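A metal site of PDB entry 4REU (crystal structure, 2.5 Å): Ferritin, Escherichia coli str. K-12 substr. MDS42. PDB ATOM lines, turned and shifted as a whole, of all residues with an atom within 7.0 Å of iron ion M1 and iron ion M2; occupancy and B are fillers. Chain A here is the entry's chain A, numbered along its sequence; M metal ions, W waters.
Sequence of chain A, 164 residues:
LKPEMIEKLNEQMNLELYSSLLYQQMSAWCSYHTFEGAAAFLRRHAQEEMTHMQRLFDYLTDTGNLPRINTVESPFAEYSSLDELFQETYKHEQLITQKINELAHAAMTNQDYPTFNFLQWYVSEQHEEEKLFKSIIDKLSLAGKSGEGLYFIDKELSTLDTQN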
ATOM      1  N   GLN A  12     -17.538   7.915   9.876  1.00  0.00           N
ATOM      2  CA  GLN A  12     -17.944   6.569  10.123  1.00  0.00           C
ATOM      3  C   GLN A  12     -16.860   5.556   9.750  1.00  0.00           C
ATOM      4  O   GLN A  12     -16.724   4.565  10.431  1.00  0.00           O
ATOM      5  CB  GLN A  12     -19.240   6.269   9.375  1.00  0.00           C
ATOM      6  CG  GLN A  12     -19.854   4.907   9.679  1.00  0.00           C
ATOM      7  CD  GLN A  12     -20.292   4.724  11.122  1.00  0.00           C
ATOM      8  OE1 GLN A  12     -20.724   5.660  11.785  1.00  0.00           O
ATOM      9  NE2 GLN A  12     -20.190   3.485  11.612  1.00  0.00           N
ATOM     10  N   LEU A  15     -14.770   5.547  12.658  1.00  0.00           N
ATOM     11  CA  LEU A  15     -15.336   4.857  13.805  1.00  0.00           C
ATOM     12  C   LEU A  15     -15.148   3.323  13.687  1.00  0.00           C
ATOM     13  O   LEU A  15     -14.871   2.638  14.675  1.00  0.00           O
ATOM     14  CB  LEU A  15     -16.806   5.212  13.975  1.00  0.00           C
ATOM     15  CG  LEU A  15     -17.531   4.559  15.160  1.00  0.00           C
ATOM     16  CD1 LEU A  15     -16.886   4.942  16.493  1.00  0.00           C
ATOM     17  CD2 LEU A  15     -18.993   4.973  15.111  1.00  0.00           C
ATOM     18  N   GLU A  16     -15.242   2.810  12.473  1.00  0.00           N
ATOM     19  CA  GLU A  16     -15.052   1.403  12.218  1.00  0.00           C
ATOM     20  C   GLU A  16     -13.606   0.959  12.421  1.00  0.00           C
ATOM     21  O   GLU A  16     -13.343  -0.169  12.849  1.00  0.00           O
ATOM     22  CB  GLU A  16     -15.514   1.053  10.813  1.00  0.00           C
ATOM     23  CG  GLU A  16     -16.967   1.413  10.540  1.00  0.00           C
ATOM     24  CD  GLU A  16     -18.005   0.381  10.985  1.00  0.00           C
ATOM     25  OE1 GLU A  16     -19.194   0.683  10.779  1.00  0.00           O
ATOM     26  OE2 GLU A  16     -17.695  -0.704  11.520  1.00  0.00           O
ATOM     27  N   SER A  19     -13.079   0.777  16.064  1.00  0.00           N
ATOM     28  CA  SER A  19     -13.764  -0.430  16.558  1.00  0.00           C
ATOM     29  C   SER A  19     -12.939  -1.686  16.356  1.00  0.00           C
ATOM     30  O   SER A  19     -12.907  -2.562  17.196  1.00  0.00           O
ATOM     31  CB  SER A  19     -15.108  -0.569  15.849  1.00  0.00           C
ATOM     32  OG  SER A  19     -15.943   0.519  16.190  1.00  0.00           O
ATOM     33  N   TYR A  23     -11.566  -3.831  19.617  1.00  0.00           N
ATOM     34  CA  TYR A  23     -11.763  -5.282  19.847  1.00  0.00           C
ATOM     35  C   TYR A  23     -10.450  -6.057  19.900  1.00  0.00           C
ATOM     36  O   TYR A  23     -10.385  -7.050  20.555  1.00  0.00           O
ATOM     37  CB  TYR A  23     -12.722  -5.927  18.778  1.00  0.00           C
ATOM     38  CG  TYR A  23     -14.106  -5.317  18.749  1.00  0.00           C
ATOM     39  CD1 TYR A  23     -14.637  -4.710  19.848  1.00  0.00           C
ATOM     40  CD2 TYR A  23     -14.865  -5.324  17.586  1.00  0.00           C
ATOM     41  CE1 TYR A  23     -15.885  -4.121  19.809  1.00  0.00           C
ATOM     42  CE2 TYR A  23     -16.139  -4.740  17.531  1.00  0.00           C
ATOM     43  CZ  TYR A  23     -16.648  -4.137  18.650  1.00  0.00           C
ATOM     44  OH  TYR A  23     -17.907  -3.549  18.672  1.00  0.00           O
ATOM     45  N   HIS A  45     -13.256 -10.732  15.220  1.00  0.00           N
ATOM     46  CA  HIS A  45     -14.192  -9.652  15.023  1.00  0.00           C
ATOM     47  C   HIS A  45     -13.512  -8.290  14.687  1.00  0.00           C
ATOM     48  O   HIS A  45     -13.994  -7.491  13.837  1.00  0.00           O
ATOM     49  CB  HIS A  45     -15.096  -9.511  16.249  1.00  0.00           C
ATOM     50  CG  HIS A  45     -16.446  -9.079  15.850  1.00  0.00           C
ATOM     51  ND1 HIS A  45     -16.829  -7.768  15.848  1.00  0.00           N
ATOM     52  CD2 HIS A  45     -17.447  -9.759  15.248  1.00  0.00           C
ATOM     53  CE1 HIS A  45     -18.038  -7.659  15.351  1.00  0.00           C
ATOM     54  NE2 HIS A  45     -18.427  -8.852  14.963  1.00  0.00           N
ATOM     55  N   GLU A  48     -13.203  -8.297  11.221  1.00  0.00           N
ATOM     56  CA  GLU A  48     -14.432  -7.906  10.593  1.00  0.00           C
ATOM     57  C   GLU A  48     -14.616  -6.389  10.532  1.00  0.00           C
ATOM     58  O   GLU A  48     -14.968  -5.862   9.464  1.00  0.00           O
ATOM     59  CB  GLU A  48     -15.634  -8.595  11.230  1.00  0.00           C
ATOM     60  CG  GLU A  48     -15.731 -10.039  10.764  1.00  0.00           C
ATOM     61  CD  GLU A  48     -16.833 -10.829  11.450  1.00  0.00           C
ATOM     62  OE1 GLU A  48     -17.976 -10.315  11.478  1.00  0.00           O
ATOM     63  OE2 GLU A  48     -16.561 -11.965  11.944  1.00  0.00           O
ATOM     64  N   GLU A  49     -14.337  -5.674  11.609  1.00  0.00           N
ATOM     65  CA  GLU A  49     -14.490  -4.221  11.592  1.00  0.00           C
ATOM     66  C   GLU A  49     -13.550  -3.539  10.610  1.00  0.00           C
ATOM     67  O   GLU A  49     -13.936  -2.585   9.938  1.00  0.00           O
ATOM     68  CB  GLU A  49     -14.287  -3.631  12.956  1.00  0.00           C
ATOM     69  CG  GLU A  49     -15.253  -4.121  14.004  1.00  0.00           C
ATOM     70  CD  GLU A  49     -16.675  -3.691  13.785  1.00  0.00           C
ATOM     71  OE1 GLU A  49     -16.935  -2.729  13.028  1.00  0.00           O
ATOM     72  OE2 GLU A  49     -17.546  -4.313  14.431  1.00  0.00           O
ATOM     73  N   MET A  50     -12.348  -4.056  10.449  1.00  0.00           N
ATOM     74  CA  MET A  50     -11.461  -3.568   9.369  1.00  0.00           C
ATOM     75  C   MET A  50     -12.138  -3.680   8.013  1.00  0.00           C
ATOM     76  O   MET A  50     -12.002  -2.785   7.194  1.00  0.00           O
ATOM     77  CB  MET A  50     -10.128  -4.301   9.360  1.00  0.00           C
ATOM     78  CG  MET A  50      -8.925  -3.443   8.986  1.00  0.00           C
ATOM     79  SD  MET A  50      -8.440  -2.096  10.117  1.00  0.00           S
ATOM     80  CE  MET A  50      -9.186  -0.823   9.147  1.00  0.00           C
ATOM     81  N   HIS A  52     -15.371  -3.568   7.406  1.00  0.00           N
ATOM     82  CA  HIS A  52     -16.342  -2.464   7.457  1.00  0.00           C
ATOM     83  C   HIS A  52     -15.680  -1.109   7.111  1.00  0.00           C
ATOM     84  O   HIS A  52     -16.190  -0.318   6.355  1.00  0.00           O
ATOM     85  CB  HIS A  52     -17.009  -2.367   8.846  1.00  0.00           C
ATOM     86  CG  HIS A  52     -17.695  -3.625   9.270  1.00  0.00           C
ATOM     87  ND1 HIS A  52     -18.360  -3.743  10.478  1.00  0.00           N
ATOM     88  CD2 HIS A  52     -17.843  -4.820   8.641  1.00  0.00           C
ATOM     89  CE1 HIS A  52     -18.862  -4.960  10.580  1.00  0.00           C
ATOM     90  NE2 HIS A  52     -18.563  -5.634   9.480  1.00  0.00           N
ATOM     91  N   MET A  53     -14.524  -0.881   7.683  1.00  0.00           N
ATOM     92  CA  MET A  53     -13.790   0.310   7.442  1.00  0.00           C
ATOM     93  C   MET A  53     -13.422   0.379   5.968  1.00  0.00           C
ATOM     94  O   MET A  53     -13.684   1.408   5.335  1.00  0.00           O
ATOM     95  CB  MET A  53     -12.579   0.326   8.365  1.00  0.00           C
ATOM     96  CG  MET A  53     -11.673   1.539   8.283  1.00  0.00           C
ATOM     97  SD  MET A  53     -10.447   1.260   6.994  1.00  0.00           S
ATOM     98  CE  MET A  53      -9.018   2.080   7.691  1.00  0.00           C
ATOM     99  N   HIS A  92     -21.031  -0.296  22.539  1.00  0.00           N
ATOM    100  CA  HIS A  92     -20.273   0.272  21.455  1.00  0.00           C
ATOM    101  C   HIS A  92     -20.988  -0.043  20.154  1.00  0.00           C
ATOM    102  O   HIS A  92     -21.221   0.841  19.350  1.00  0.00           O
ATOM    103  CB  HIS A  92     -18.822  -0.150  21.499  1.00  0.00           C
ATOM    104  CG  HIS A  92     -17.968   0.516  20.460  1.00  0.00           C
ATOM    105  ND1 HIS A  92     -17.538   1.820  20.584  1.00  0.00           N
ATOM    106  CD2 HIS A  92     -17.535   0.084  19.258  1.00  0.00           C
ATOM    107  CE1 HIS A  92     -16.839   2.138  19.511  1.00  0.00           C
ATOM    108  NE2 HIS A  92     -16.822   1.104  18.684  1.00  0.00           N
ATOM    109  N   GLU A  93     -21.412  -1.265  19.975  1.00  0.00           N
ATOM    110  CA  GLU A  93     -22.104  -1.587  18.723  1.00  0.00           C
ATOM    111  C   GLU A  93     -23.395  -0.824  18.611  1.00  0.00           C
ATOM    112  O   GLU A  93     -23.833  -0.563  17.503  1.00  0.00           O
ATOM    113  CB  GLU A  93     -22.339  -3.080  18.537  1.00  0.00           C
ATOM    114  CG  GLU A  93     -21.081  -3.835  18.222  1.00  0.00           C
ATOM    115  CD  GLU A  93     -20.620  -3.732  16.799  1.00  0.00           C
ATOM    116  OE1 GLU A  93     -19.412  -3.926  16.533  1.00  0.00           O
ATOM    117  OE2 GLU A  93     -21.453  -3.507  15.906  1.00  0.00           O
ATOM    118  N   ILE A  96     -22.516   2.500  17.132  1.00  0.00           N
ATOM    119  CA  ILE A  96     -22.251   2.336  15.709  1.00  0.00           C
ATOM    120  C   ILE A  96     -23.567   2.275  14.964  1.00  0.00           C
ATOM    121  O   ILE A  96     -23.738   2.909  13.934  1.00  0.00           O
ATOM    122  CB  ILE A  96     -21.473   1.029  15.460  1.00  0.00           C
ATOM    123  CG1 ILE A  96     -20.049   1.197  15.938  1.00  0.00           C
ATOM    124  CG2 ILE A  96     -21.459   0.640  13.998  1.00  0.00           C
ATOM    125  CD1 ILE A  96     -19.272  -0.086  15.977  1.00  0.00           C
ATOM    126  N   TRP A 121     -26.376  -1.936   3.644  1.00  0.00           N
ATOM    127  CA  TRP A 121     -25.538  -3.064   4.013  1.00  0.00           C
ATOM    128  C   TRP A 121     -25.107  -2.959   5.489  1.00  0.00           C
ATOM    129  O   TRP A 121     -24.939  -3.948   6.179  1.00  0.00           O
ATOM    130  CB  TRP A 121     -24.285  -3.088   3.097  1.00  0.00           C
ATOM    131  CG  TRP A 121     -23.464  -4.272   3.319  1.00  0.00           C
ATOM    132  CD1 TRP A 121     -23.518  -5.429   2.632  1.00  0.00           C
ATOM    133  CD2 TRP A 121     -22.485  -4.458   4.358  1.00  0.00           C
ATOM    134  NE1 TRP A 121     -22.630  -6.344   3.167  1.00  0.00           N
ATOM    135  CE2 TRP A 121     -21.982  -5.771   4.232  1.00  0.00           C
ATOM    136  CE3 TRP A 121     -21.958  -3.623   5.364  1.00  0.00           C
ATOM    137  CZ2 TRP A 121     -20.979  -6.287   5.060  1.00  0.00           C
ATOM    138  CZ3 TRP A 121     -20.972  -4.127   6.213  1.00  0.00           C
ATOM    139  CH2 TRP A 121     -20.492  -5.452   6.050  1.00  0.00           C
ATOM    140  N   TYR A 122     -24.842  -1.741   5.920  1.00  0.00           N
ATOM    141  CA  TYR A 122     -24.490  -1.471   7.286  1.00  0.00           C
ATOM    142  C   TYR A 122     -25.717  -1.608   8.174  1.00  0.00           C
ATOM    143  O   TYR A 122     -25.620  -2.099   9.302  1.00  0.00           O
ATOM    144  CB  TYR A 122     -23.874  -0.060   7.410  1.00  0.00           C
ATOM    145  CG  TYR A 122     -22.474   0.014   6.852  1.00  0.00           C
ATOM    146  CD1 TYR A 122     -22.262   0.337   5.530  1.00  0.00           C
ATOM    147  CD2 TYR A 122     -21.347  -0.223   7.660  1.00  0.00           C
ATOM    148  CE1 TYR A 122     -20.995   0.379   5.000  1.00  0.00           C
ATOM    149  CE2 TYR A 122     -20.082  -0.203   7.127  1.00  0.00           C
ATOM    150  CZ  TYR A 122     -19.916   0.101   5.794  1.00  0.00           C
ATOM    151  OH  TYR A 122     -18.678   0.157   5.192  1.00  0.00           O
ATOM    152  N   GLU A 125     -26.230  -5.236   8.631  1.00  0.00           N
ATOM    153  CA  GLU A 125     -25.099  -5.710   9.423  1.00  0.00           C
ATOM    154  C   GLU A 125     -25.161  -5.343  10.860  1.00  0.00           C
ATOM    155  O   GLU A 125     -24.796  -6.147  11.692  1.00  0.00           O
ATOM    156  CB  GLU A 125     -23.762  -5.256   8.882  1.00  0.00           C
ATOM    157  CG  GLU A 125     -23.108  -6.354   8.051  1.00  0.00           C
ATOM    158  CD  GLU A 125     -22.517  -7.457   8.906  1.00  0.00           C
ATOM    159  OE1 GLU A 125     -22.671  -8.631   8.507  1.00  0.00           O
ATOM    160  OE2 GLU A 125     -21.907  -7.115   9.961  1.00  0.00           O
ATOM    161  N   GLN A 126     -25.592  -4.130  11.164  1.00  0.00           N
ATOM    162  CA  GLN A 126     -25.682  -3.710  12.550  1.00  0.00           C
ATOM    163  C   GLN A 126     -26.757  -4.465  13.320  1.00  0.00           C
ATOM    164  O   GLN A 126     -26.604  -4.744  14.497  1.00  0.00           O
ATOM    165  CB  GLN A 126     -25.903  -2.199  12.656  1.00  0.00           C
ATOM    166  CG  GLN A 126     -24.623  -1.416  12.396  1.00  0.00           C
ATOM    167  CD  GLN A 126     -23.457  -1.906  13.223  1.00  0.00           C
ATOM    168  OE1 GLN A 126     -22.471  -2.365  12.688  1.00  0.00           O
ATOM    169  NE2 GLN A 126     -23.572  -1.805  14.534  1.00  0.00           N
ATOM    170  N   GLU A 129     -25.004  -7.577  14.222  1.00  0.00           N
ATOM    171  CA  GLU A 129     -24.047  -7.280  15.263  1.00  0.00           C
ATOM    172  C   GLU A 129     -24.738  -7.125  16.629  1.00  0.00           C
ATOM    173  O   GLU A 129     -24.215  -7.598  17.644  1.00  0.00           O
ATOM    174  CB  GLU A 129     -23.261  -6.004  14.959  1.00  0.00           C
ATOM    175  CG  GLU A 129     -22.426  -6.043  13.693  1.00  0.00           C
ATOM    176  CD  GLU A 129     -21.142  -6.785  13.911  1.00  0.00           C
ATOM    177  OE1 GLU A 129     -21.126  -8.016  13.660  1.00  0.00           O
ATOM    178  OE2 GLU A 129     -20.190  -6.127  14.364  1.00  0.00           O
ATOM    179  N   PHE A 133     -23.829  -9.767  19.854  1.00  0.00           N
ATOM    180  CA  PHE A 133     -23.284  -9.257  21.110  1.00  0.00           C
ATOM    181  C   PHE A 133     -24.311  -9.341  22.270  1.00  0.00           C
ATOM    182  O   PHE A 133     -23.927  -9.680  23.381  1.00  0.00           O
ATOM    183  CB  PHE A 133     -22.677  -7.859  20.931  1.00  0.00           C
ATOM    184  CG  PHE A 133     -21.331  -7.873  20.217  1.00  0.00           C
ATOM    185  CD1 PHE A 133     -20.140  -8.028  20.932  1.00  0.00           C
ATOM    186  CD2 PHE A 133     -21.252  -7.761  18.829  1.00  0.00           C
ATOM    187  CE1 PHE A 133     -18.907  -8.051  20.274  1.00  0.00           C
ATOM    188  CE2 PHE A 133     -20.028  -7.789  18.181  1.00  0.00           C
ATOM    189  CZ  PHE A 133     -18.848  -7.935  18.910  1.00  0.00           C
HETATM  190 FE    FE M   1     -18.630  -2.315  12.006  1.00  0.00          FE
HETATM  191 FE    FE M   2     -19.401  -4.172  14.661  1.00  0.00          FE
HETATM  192  O   HOH W   1     -20.045  -2.806  13.524  1.00  0.00           O
HETATM  193  O   HOH W   2     -20.400  -1.486  10.863  1.00  0.00           O
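A ring nitrogen (NE2) of His 45 is in hydrogen-bond range of the side-chain carboxylate (OE1) of Glu 129 (3.1 Å).
The side-chain hydroxyl (OH) of Tyr 122 is in hydrogen-bond range of the backbone carbonyl oxygen (O) of His 52, at 2.8 Å.
The side-chain carboxylate (OE1) of Glu 93 lies close to the side-chain hydroxyl (OH) of Tyr 23, at 2.6 Å.
The side-chain amide nitrogen (NE2) of Gln 126 lies within hydrogen-bond range of the backbone carbonyl oxygen (O) of Glu 93.
The side-chain amide nitrogen of Gln 12 lies within hydrogen-bond range of the side-chain carboxylate of Glu 16 (3.1 Å).
Merely in contact with iron ion M2: His 45.
The side-chain carboxylate (OE2) of Glu 49 binds iron ion M2, at 1.9 Å.
Iron ion M2 is bound by the side-chain carboxylate (OE1) of Glu 93, 1.9 Å away.
Water W1 is bound to iron ion M2 (1.9 Å).
OE2 of Glu 129 binds iron ion M2, 2.1 Å away.
Iron ion M2 is bound by OE2 of Glu 93, 2.5 Å away.
Water W2 lies within hydrogen-bond range of the side-chain carboxylate (OE1) of Glu 16 (2.5 Å) and the side-chain amide oxygen (OE1) of Gln 126 (2.9 Å).
Merely in contact with iron ion M1: Gln 126.
Iron ion M1 is bound by the side-chain carboxylate (OE2) of Glu 16, the side-chain carboxylate (OE1) of Glu 49, a ring nitrogen (ND1) of His 52, water W1 and water W2.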
